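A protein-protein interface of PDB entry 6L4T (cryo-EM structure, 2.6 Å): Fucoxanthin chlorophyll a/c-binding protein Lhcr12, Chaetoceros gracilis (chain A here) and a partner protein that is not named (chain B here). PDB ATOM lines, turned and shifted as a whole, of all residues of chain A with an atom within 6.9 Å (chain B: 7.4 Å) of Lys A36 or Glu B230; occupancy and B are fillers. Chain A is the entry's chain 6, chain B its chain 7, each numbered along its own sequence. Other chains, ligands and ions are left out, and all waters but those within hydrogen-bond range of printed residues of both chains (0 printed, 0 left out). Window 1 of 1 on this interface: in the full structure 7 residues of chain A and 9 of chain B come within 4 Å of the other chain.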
ATOM      1  N   LYS A  35     -28.540  14.727  -3.230  1.00  0.00           N
ATOM      2  CA  LYS A  35     -27.503  15.751  -3.213  1.00  0.00           C
ATOM      3  C   LYS A  35     -28.114  17.129  -3.067  1.00  0.00           C
ATOM      4  O   LYS A  35     -29.225  17.357  -3.552  1.00  0.00           O
ATOM      5  CB  LYS A  35     -26.665  15.689  -4.487  1.00  0.00           C
ATOM      6  CG  LYS A  35     -25.991  14.355  -4.714  1.00  0.00           C
ATOM      7  CD  LYS A  35     -24.856  14.482  -5.708  1.00  0.00           C
ATOM      8  CE  LYS A  35     -23.713  15.294  -5.131  1.00  0.00           C
ATOM      9  NZ  LYS A  35     -22.570  15.357  -6.078  1.00  0.00           N
ATOM     10  N   LYS A  36     -27.374  18.029  -2.408  1.00  0.00           N
ATOM     11  CA  LYS A  36     -27.744  19.435  -2.218  1.00  0.00           C
ATOM     12  C   LYS A  36     -29.077  19.563  -1.473  1.00  0.00           C
ATOM     13  O   LYS A  36     -30.140  19.754  -2.070  1.00  0.00           O
ATOM     14  CB  LYS A  36     -27.748  20.203  -3.544  1.00  0.00           C
ATOM     15  CG  LYS A  36     -26.387  20.258  -4.225  1.00  0.00           C
ATOM     16  CD  LYS A  36     -25.435  21.215  -3.527  1.00  0.00           C
ATOM     17  CE  LYS A  36     -24.281  20.479  -2.856  1.00  0.00           C
ATOM     18  NZ  LYS A  36     -23.290  21.412  -2.248  1.00  0.00           N
ATOM     19  N   SER A  37     -28.971  19.306  -0.161  1.00  0.00           N
ATOM     20  CA  SER A  37     -30.015  19.515   0.845  1.00  0.00           C
ATOM     21  C   SER A  37     -30.851  20.761   0.595  1.00  0.00           C
ATOM     22  O   SER A  37     -30.328  21.822   0.264  1.00  0.00           O
ATOM     23  CB  SER A  37     -29.359  19.628   2.221  1.00  0.00           C
ATOM     24  OG  SER A  37     -30.284  20.069   3.191  1.00  0.00           O
ATOM     25  N   GLN A  38     -32.166  20.611   0.752  1.00  0.00           N
ATOM     26  CA  GLN A  38     -33.096  21.655   0.336  1.00  0.00           C
ATOM     27  C   GLN A  38     -33.053  22.854   1.273  1.00  0.00           C
ATOM     28  O   GLN A  38     -33.026  24.002   0.816  1.00  0.00           O
ATOM     29  CB  GLN A  38     -34.506  21.081   0.261  1.00  0.00           C
ATOM     30  CG  GLN A  38     -35.598  22.113   0.147  1.00  0.00           C
ATOM     31  CD  GLN A  38     -36.951  21.480   0.022  1.00  0.00           C
ATOM     32  OE1 GLN A  38     -37.122  20.299   0.307  1.00  0.00           O
ATOM     33  NE2 GLN A  38     -37.929  22.260  -0.412  1.00  0.00           N
ATOM     34  N   ALA A  39     -33.039  22.606   2.582  1.00  0.00           N
ATOM     35  CA  ALA A  39     -32.996  23.690   3.554  1.00  0.00           C
ATOM     36  C   ALA A  39     -31.662  24.414   3.534  1.00  0.00           C
ATOM     37  O   ALA A  39     -31.611  25.625   3.776  1.00  0.00           O
ATOM     38  CB  ALA A  39     -33.261  23.144   4.952  1.00  0.00           C
ATOM     39  N   LEU A  40     -30.582  23.692   3.259  1.00  0.00           N
ATOM     40  CA  LEU A  40     -29.224  24.225   3.283  1.00  0.00           C
ATOM     41  C   LEU A  40     -28.599  23.893   1.938  1.00  0.00           C
ATOM     42  O   LEU A  40     -27.893  22.886   1.809  1.00  0.00           O
ATOM     43  CB  LEU A  40     -28.425  23.615   4.429  1.00  0.00           C
ATOM     44  CG  LEU A  40     -29.013  23.857   5.816  1.00  0.00           C
ATOM     45  CD1 LEU A  40     -28.314  23.032   6.857  1.00  0.00           C
ATOM     46  CD2 LEU A  40     -28.901  25.308   6.158  1.00  0.00           C
ATOM     47  N   PRO A  41     -28.832  24.719   0.912  1.00  0.00           N
ATOM     48  CA  PRO A  41     -28.389  24.363  -0.448  1.00  0.00           C
ATOM     49  C   PRO A  41     -26.885  24.398  -0.647  1.00  0.00           C
ATOM     50  O   PRO A  41     -26.404  23.905  -1.674  1.00  0.00           O
ATOM     51  CB  PRO A  41     -29.088  25.407  -1.323  1.00  0.00           C
ATOM     52  CG  PRO A  41     -29.319  26.550  -0.422  1.00  0.00           C
ATOM     53  CD  PRO A  41     -29.584  25.983   0.930  1.00  0.00           C
ATOM     54  N   PHE A  42     -26.137  24.950   0.295  1.00  0.00           N
ATOM     55  CA  PHE A  42     -24.686  24.974   0.267  1.00  0.00           C
ATOM     56  C   PHE A  42     -24.072  23.746   0.922  1.00  0.00           C
ATOM     57  O   PHE A  42     -22.845  23.643   0.990  1.00  0.00           O
ATOM     58  CB  PHE A  42     -24.176  26.243   0.957  1.00  0.00           C
ATOM     59  CG  PHE A  42     -24.922  26.595   2.217  1.00  0.00           C
ATOM     60  CD1 PHE A  42     -24.560  26.034   3.424  1.00  0.00           C
ATOM     61  CD2 PHE A  42     -25.968  27.501   2.196  1.00  0.00           C
ATOM     62  CE1 PHE A  42     -25.231  26.350   4.576  1.00  0.00           C
ATOM     63  CE2 PHE A  42     -26.647  27.815   3.347  1.00  0.00           C
ATOM     64  CZ  PHE A  42     -26.272  27.243   4.539  1.00  0.00           C
ATOM     65  N   LEU A  43     -24.895  22.820   1.401  1.00  0.00           N
ATOM     66  CA  LEU A  43     -24.472  21.627   2.104  1.00  0.00           C
ATOM     67  C   LEU A  43     -24.998  20.388   1.394  1.00  0.00           C
ATOM     68  O   LEU A  43     -26.076  20.430   0.793  1.00  0.00           O
ATOM     69  CB  LEU A  43     -24.978  21.646   3.551  1.00  0.00           C
ATOM     70  CG  LEU A  43     -24.024  22.281   4.559  1.00  0.00           C
ATOM     71  CD1 LEU A  43     -24.765  22.756   5.777  1.00  0.00           C
ATOM     72  CD2 LEU A  43     -22.979  21.283   4.959  1.00  0.00           C
ATOM     73  N   PRO A  44     -24.261  19.280   1.425  1.00  0.00           N
ATOM     74  CA  PRO A  44     -24.763  18.047   0.815  1.00  0.00           C
ATOM     75  C   PRO A  44     -25.894  17.442   1.627  1.00  0.00           C
ATOM     76  O   PRO A  44     -26.072  17.722   2.813  1.00  0.00           O
ATOM     77  CB  PRO A  44     -23.536  17.132   0.806  1.00  0.00           C
ATOM     78  CG  PRO A  44     -22.693  17.638   1.908  1.00  0.00           C
ATOM     79  CD  PRO A  44     -22.877  19.123   1.901  1.00  0.00           C
ATOM     80  N   TYR A  45     -26.660  16.597   0.965  1.00  0.00           N
ATOM     81  CA  TYR A  45     -27.859  16.037   1.572  1.00  0.00           C
ATOM     82  C   TYR A  45     -27.491  14.874   2.485  1.00  0.00           C
ATOM     83  O   TYR A  45     -26.807  13.945   2.046  1.00  0.00           O
ATOM     84  CB  TYR A  45     -28.821  15.572   0.489  1.00  0.00           C
ATOM     85  CG  TYR A  45     -30.079  14.923   1.003  1.00  0.00           C
ATOM     86  CD1 TYR A  45     -31.104  15.686   1.540  1.00  0.00           C
ATOM     87  CD2 TYR A  45     -30.249  13.548   0.936  1.00  0.00           C
ATOM     88  CE1 TYR A  45     -32.259  15.097   2.007  1.00  0.00           C
ATOM     89  CE2 TYR A  45     -31.395  12.951   1.402  1.00  0.00           C
ATOM     90  CZ  TYR A  45     -32.397  13.729   1.935  1.00  0.00           C
ATOM     91  OH  TYR A  45     -33.545  13.134   2.396  1.00  0.00           O
ATOM     92  N   TYR B 149      -8.556  27.201   0.229  1.00  0.00           N
ATOM     93  CA  TYR B 149     -10.007  27.224   0.385  1.00  0.00           C
ATOM     94  C   TYR B 149     -10.409  27.875   1.699  1.00  0.00           C
ATOM     95  O   TYR B 149     -11.376  28.641   1.745  1.00  0.00           O
ATOM     96  CB  TYR B 149     -10.560  25.801   0.308  1.00  0.00           C
ATOM     97  CG  TYR B 149     -12.057  25.691   0.096  1.00  0.00           C
ATOM     98  CD1 TYR B 149     -12.950  25.836   1.149  1.00  0.00           C
ATOM     99  CD2 TYR B 149     -12.572  25.406  -1.153  1.00  0.00           C
ATOM    100  CE1 TYR B 149     -14.301  25.734   0.960  1.00  0.00           C
ATOM    101  CE2 TYR B 149     -13.926  25.287  -1.349  1.00  0.00           C
ATOM    102  CZ  TYR B 149     -14.785  25.458  -0.290  1.00  0.00           C
ATOM    103  OH  TYR B 149     -16.138  25.349  -0.478  1.00  0.00           O
ATOM    104  N   GLN B 224     -16.982  20.597   4.626  1.00  0.00           N
ATOM    105  CA  GLN B 224     -17.530  19.613   3.702  1.00  0.00           C
ATOM    106  C   GLN B 224     -17.441  20.096   2.264  1.00  0.00           C
ATOM    107  O   GLN B 224     -17.338  19.278   1.346  1.00  0.00           O
ATOM    108  CB  GLN B 224     -18.974  19.275   4.068  1.00  0.00           C
ATOM    109  CG  GLN B 224     -19.087  18.027   4.919  1.00  0.00           C
ATOM    110  CD  GLN B 224     -20.360  17.973   5.730  1.00  0.00           C
ATOM    111  OE1 GLN B 224     -21.419  18.401   5.277  1.00  0.00           O
ATOM    112  NE2 GLN B 224     -20.263  17.440   6.941  1.00  0.00           N
ATOM    113  N   GLY B 225     -17.465  21.407   2.047  1.00  0.00           N
ATOM    114  CA  GLY B 225     -17.261  21.940   0.717  1.00  0.00           C
ATOM    115  C   GLY B 225     -15.834  21.869   0.233  1.00  0.00           C
ATOM    116  O   GLY B 225     -15.595  22.018  -0.968  1.00  0.00           O
ATOM    117  N   ARG B 226     -14.888  21.638   1.136  1.00  0.00           N
ATOM    118  CA  ARG B 226     -13.476  21.559   0.805  1.00  0.00           C
ATOM    119  C   ARG B 226     -13.035  20.134   0.495  1.00  0.00           C
ATOM    120  O   ARG B 226     -12.298  19.914  -0.471  1.00  0.00           O
ATOM    121  CB  ARG B 226     -12.658  22.136   1.961  1.00  0.00           C
ATOM    122  CG  ARG B 226     -11.204  21.787   1.953  1.00  0.00           C
ATOM    123  CD  ARG B 226     -10.469  22.648   2.933  1.00  0.00           C
ATOM    124  NE  ARG B 226     -11.016  22.563   4.279  1.00  0.00           N
ATOM    125  CZ  ARG B 226     -10.360  22.952   5.365  1.00  0.00           C
ATOM    126  NH1 ARG B 226      -9.139  23.448   5.257  1.00  0.00           N
ATOM    127  NH2 ARG B 226     -10.922  22.845   6.558  1.00  0.00           N
ATOM    128  N   GLU B 227     -13.475  19.157   1.295  1.00  0.00           N
ATOM    129  CA  GLU B 227     -13.156  17.762   1.005  1.00  0.00           C
ATOM    130  C   GLU B 227     -13.886  17.273  -0.236  1.00  0.00           C
ATOM    131  O   GLU B 227     -13.370  16.417  -0.962  1.00  0.00           O
ATOM    132  CB  GLU B 227     -13.486  16.879   2.208  1.00  0.00           C
ATOM    133  CG  GLU B 227     -12.875  17.361   3.514  1.00  0.00           C
ATOM    134  CD  GLU B 227     -13.084  16.387   4.660  1.00  0.00           C
ATOM    135  OE1 GLU B 227     -12.625  16.679   5.785  1.00  0.00           O
ATOM    136  OE2 GLU B 227     -13.705  15.328   4.434  1.00  0.00           O
ATOM    137  N   SER B 228     -15.068  17.809  -0.503  1.00  0.00           N
ATOM    138  CA  SER B 228     -15.738  17.617  -1.776  1.00  0.00           C
ATOM    139  C   SER B 228     -15.245  18.673  -2.763  1.00  0.00           C
ATOM    140  O   SER B 228     -14.225  19.333  -2.549  1.00  0.00           O
ATOM    141  CB  SER B 228     -17.249  17.680  -1.592  1.00  0.00           C
ATOM    142  OG  SER B 228     -17.905  17.567  -2.838  1.00  0.00           O
ATOM    143  N   GLY B 229     -15.953  18.839  -3.869  1.00  0.00           N
ATOM    144  CA  GLY B 229     -15.626  19.914  -4.782  1.00  0.00           C
ATOM    145  C   GLY B 229     -16.851  20.693  -5.199  1.00  0.00           C
ATOM    146  O   GLY B 229     -16.791  21.513  -6.118  1.00  0.00           O
ATOM    147  N   GLU B 230     -17.970  20.455  -4.519  1.00  0.00           N
ATOM    148  CA  GLU B 230     -19.265  20.960  -4.946  1.00  0.00           C
ATOM    149  C   GLU B 230     -19.640  22.280  -4.290  1.00  0.00           C
ATOM    150  O   GLU B 230     -20.830  22.603  -4.215  1.00  0.00           O
ATOM    151  CB  GLU B 230     -20.347  19.915  -4.672  1.00  0.00           C
ATOM    152  CG  GLU B 230     -20.240  18.684  -5.551  1.00  0.00           C
ATOM    153  CD  GLU B 230     -20.382  17.398  -4.767  1.00  0.00           C
ATOM    154  OE1 GLU B 230     -19.795  16.379  -5.184  1.00  0.00           O
ATOM    155  OE2 GLU B 230     -21.080  17.407  -3.732  1.00  0.00           O
ATOM    156  N   ARG B 231     -18.663  23.053  -3.823  1.00  0.00           N
ATOM    157  CA  ARG B 231     -18.947  24.363  -3.249  1.00  0.00           C
ATOM    158  C   ARG B 231     -17.728  25.250  -3.413  1.00  0.00           C
ATOM    159  O   ARG B 231     -16.638  24.890  -2.965  1.00  0.00           O
ATOM    160  CB  ARG B 231     -19.330  24.257  -1.774  1.00  0.00           C
ATOM    161  CG  ARG B 231     -19.832  25.560  -1.193  1.00  0.00           C
ATOM    162  CD  ARG B 231     -19.897  25.508   0.315  1.00  0.00           C
ATOM    163  NE  ARG B 231     -20.142  26.824   0.889  1.00  0.00           N
ATOM    164  CZ  ARG B 231     -19.197  27.592   1.416  1.00  0.00           C
ATOM    165  NH1 ARG B 231     -19.508  28.776   1.917  1.00  0.00           N
ATOM    166  NH2 ARG B 231     -17.944  27.175   1.442  1.00  0.00           N
ATOM    167  N   ALA B 232     -17.911  26.392  -4.066  1.00  0.00           N
ATOM    168  CA  ALA B 232     -16.886  27.419  -4.080  1.00  0.00           C
ATOM    169  C   ALA B 232     -16.793  28.054  -2.694  1.00  0.00           C
ATOM    170  O   ALA B 232     -17.773  28.059  -1.947  1.00  0.00           O
ATOM    171  CB  ALA B 232     -17.218  28.475  -5.131  1.00  0.00           C
ATOM    172  N   ASP B 235     -19.508  30.611  -1.167  1.00  0.00           N
ATOM    173  CA  ASP B 235     -20.746  30.394  -1.900  1.00  0.00           C
ATOM    174  C   ASP B 235     -21.784  29.807  -0.957  1.00  0.00           C
ATOM    175  O   ASP B 235     -21.560  28.751  -0.359  1.00  0.00           O
ATOM    176  CB  ASP B 235     -20.502  29.462  -3.085  1.00  0.00           C
ATOM    177  CG  ASP B 235     -21.649  29.445  -4.073  1.00  0.00           C
ATOM    178  OD1 ASP B 235     -22.642  30.171  -3.876  1.00  0.00           O
ATOM    179  OD2 ASP B 235     -21.551  28.688  -5.060  1.00  0.00           O
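NZ of Lys A35 is in salt-bridge range of OE1 of Glu B230, at 3.1 Å.
The backbone carbonyl oxygen (O) of Glu B230 is in hydrogen-bond range of the side-chain amino group (NZ) of Lys A36, 3.4 Å away.
O of Leu A43 lies within hydrogen-bond range of N of Ser A37 (3.2 Å).
OH of Tyr B149 sits at hydrogen-bond distance from O of Arg B231, at 2.6 Å.
OE1 of Glu B230 lies close to OG of Ser B228 (3.2 Å).
The backbone carbonyl oxygen (O) of Asp B235 sits at hydrogen-bond distance from the guanidinium group (NE) of Arg B231 (2.7 Å).
Among the printed residues, merely in contact across the chains: Leu A43 with Gln B224 (3.3 Å), Phe A42 with Arg B231 (3.6 Å), Pro A44 with Gln B224 (3.7 Å) and Phe A42 with Asp B235 (3.9 Å).
Of the printed residues of chain B, Lys A35 touches Glu B230.
Of chain B, only Glu B230 comes within 4 Å of Lys A36.
Of the printed residues of chain B, Phe A42 touches Arg B231 (3.6 Å) and Asp B235 (3.9 Å).
Of the printed residues of chain B, Leu A43 touches Gln B224 (3.3 Å).
Of the printed residues of chain B, Pro A44 touches Gln B224.
Glu B230 touches just these residues of chain A: Lys A35 and Lys A36.
Of the printed residues of chain A, Asp B235 touches Phe A42.
The nearest residue of chain B that does not touch Lys A36 is Arg B231 (4.9 Å).
The nearest residue of chain A that does not touch Glu B230 is Pro A44 (5.2 Å).
Hydrophobic or aromatic side chains of chain A within 4 Å of the printed part of chain B: Phe A42, Leu A43 and Pro A44.
Among the printed residues, Asp or Glu carboxylates within 4 Å of a Lys or Arg side-chain nitrogen of the other chain: Lys A35 with Glu B230.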
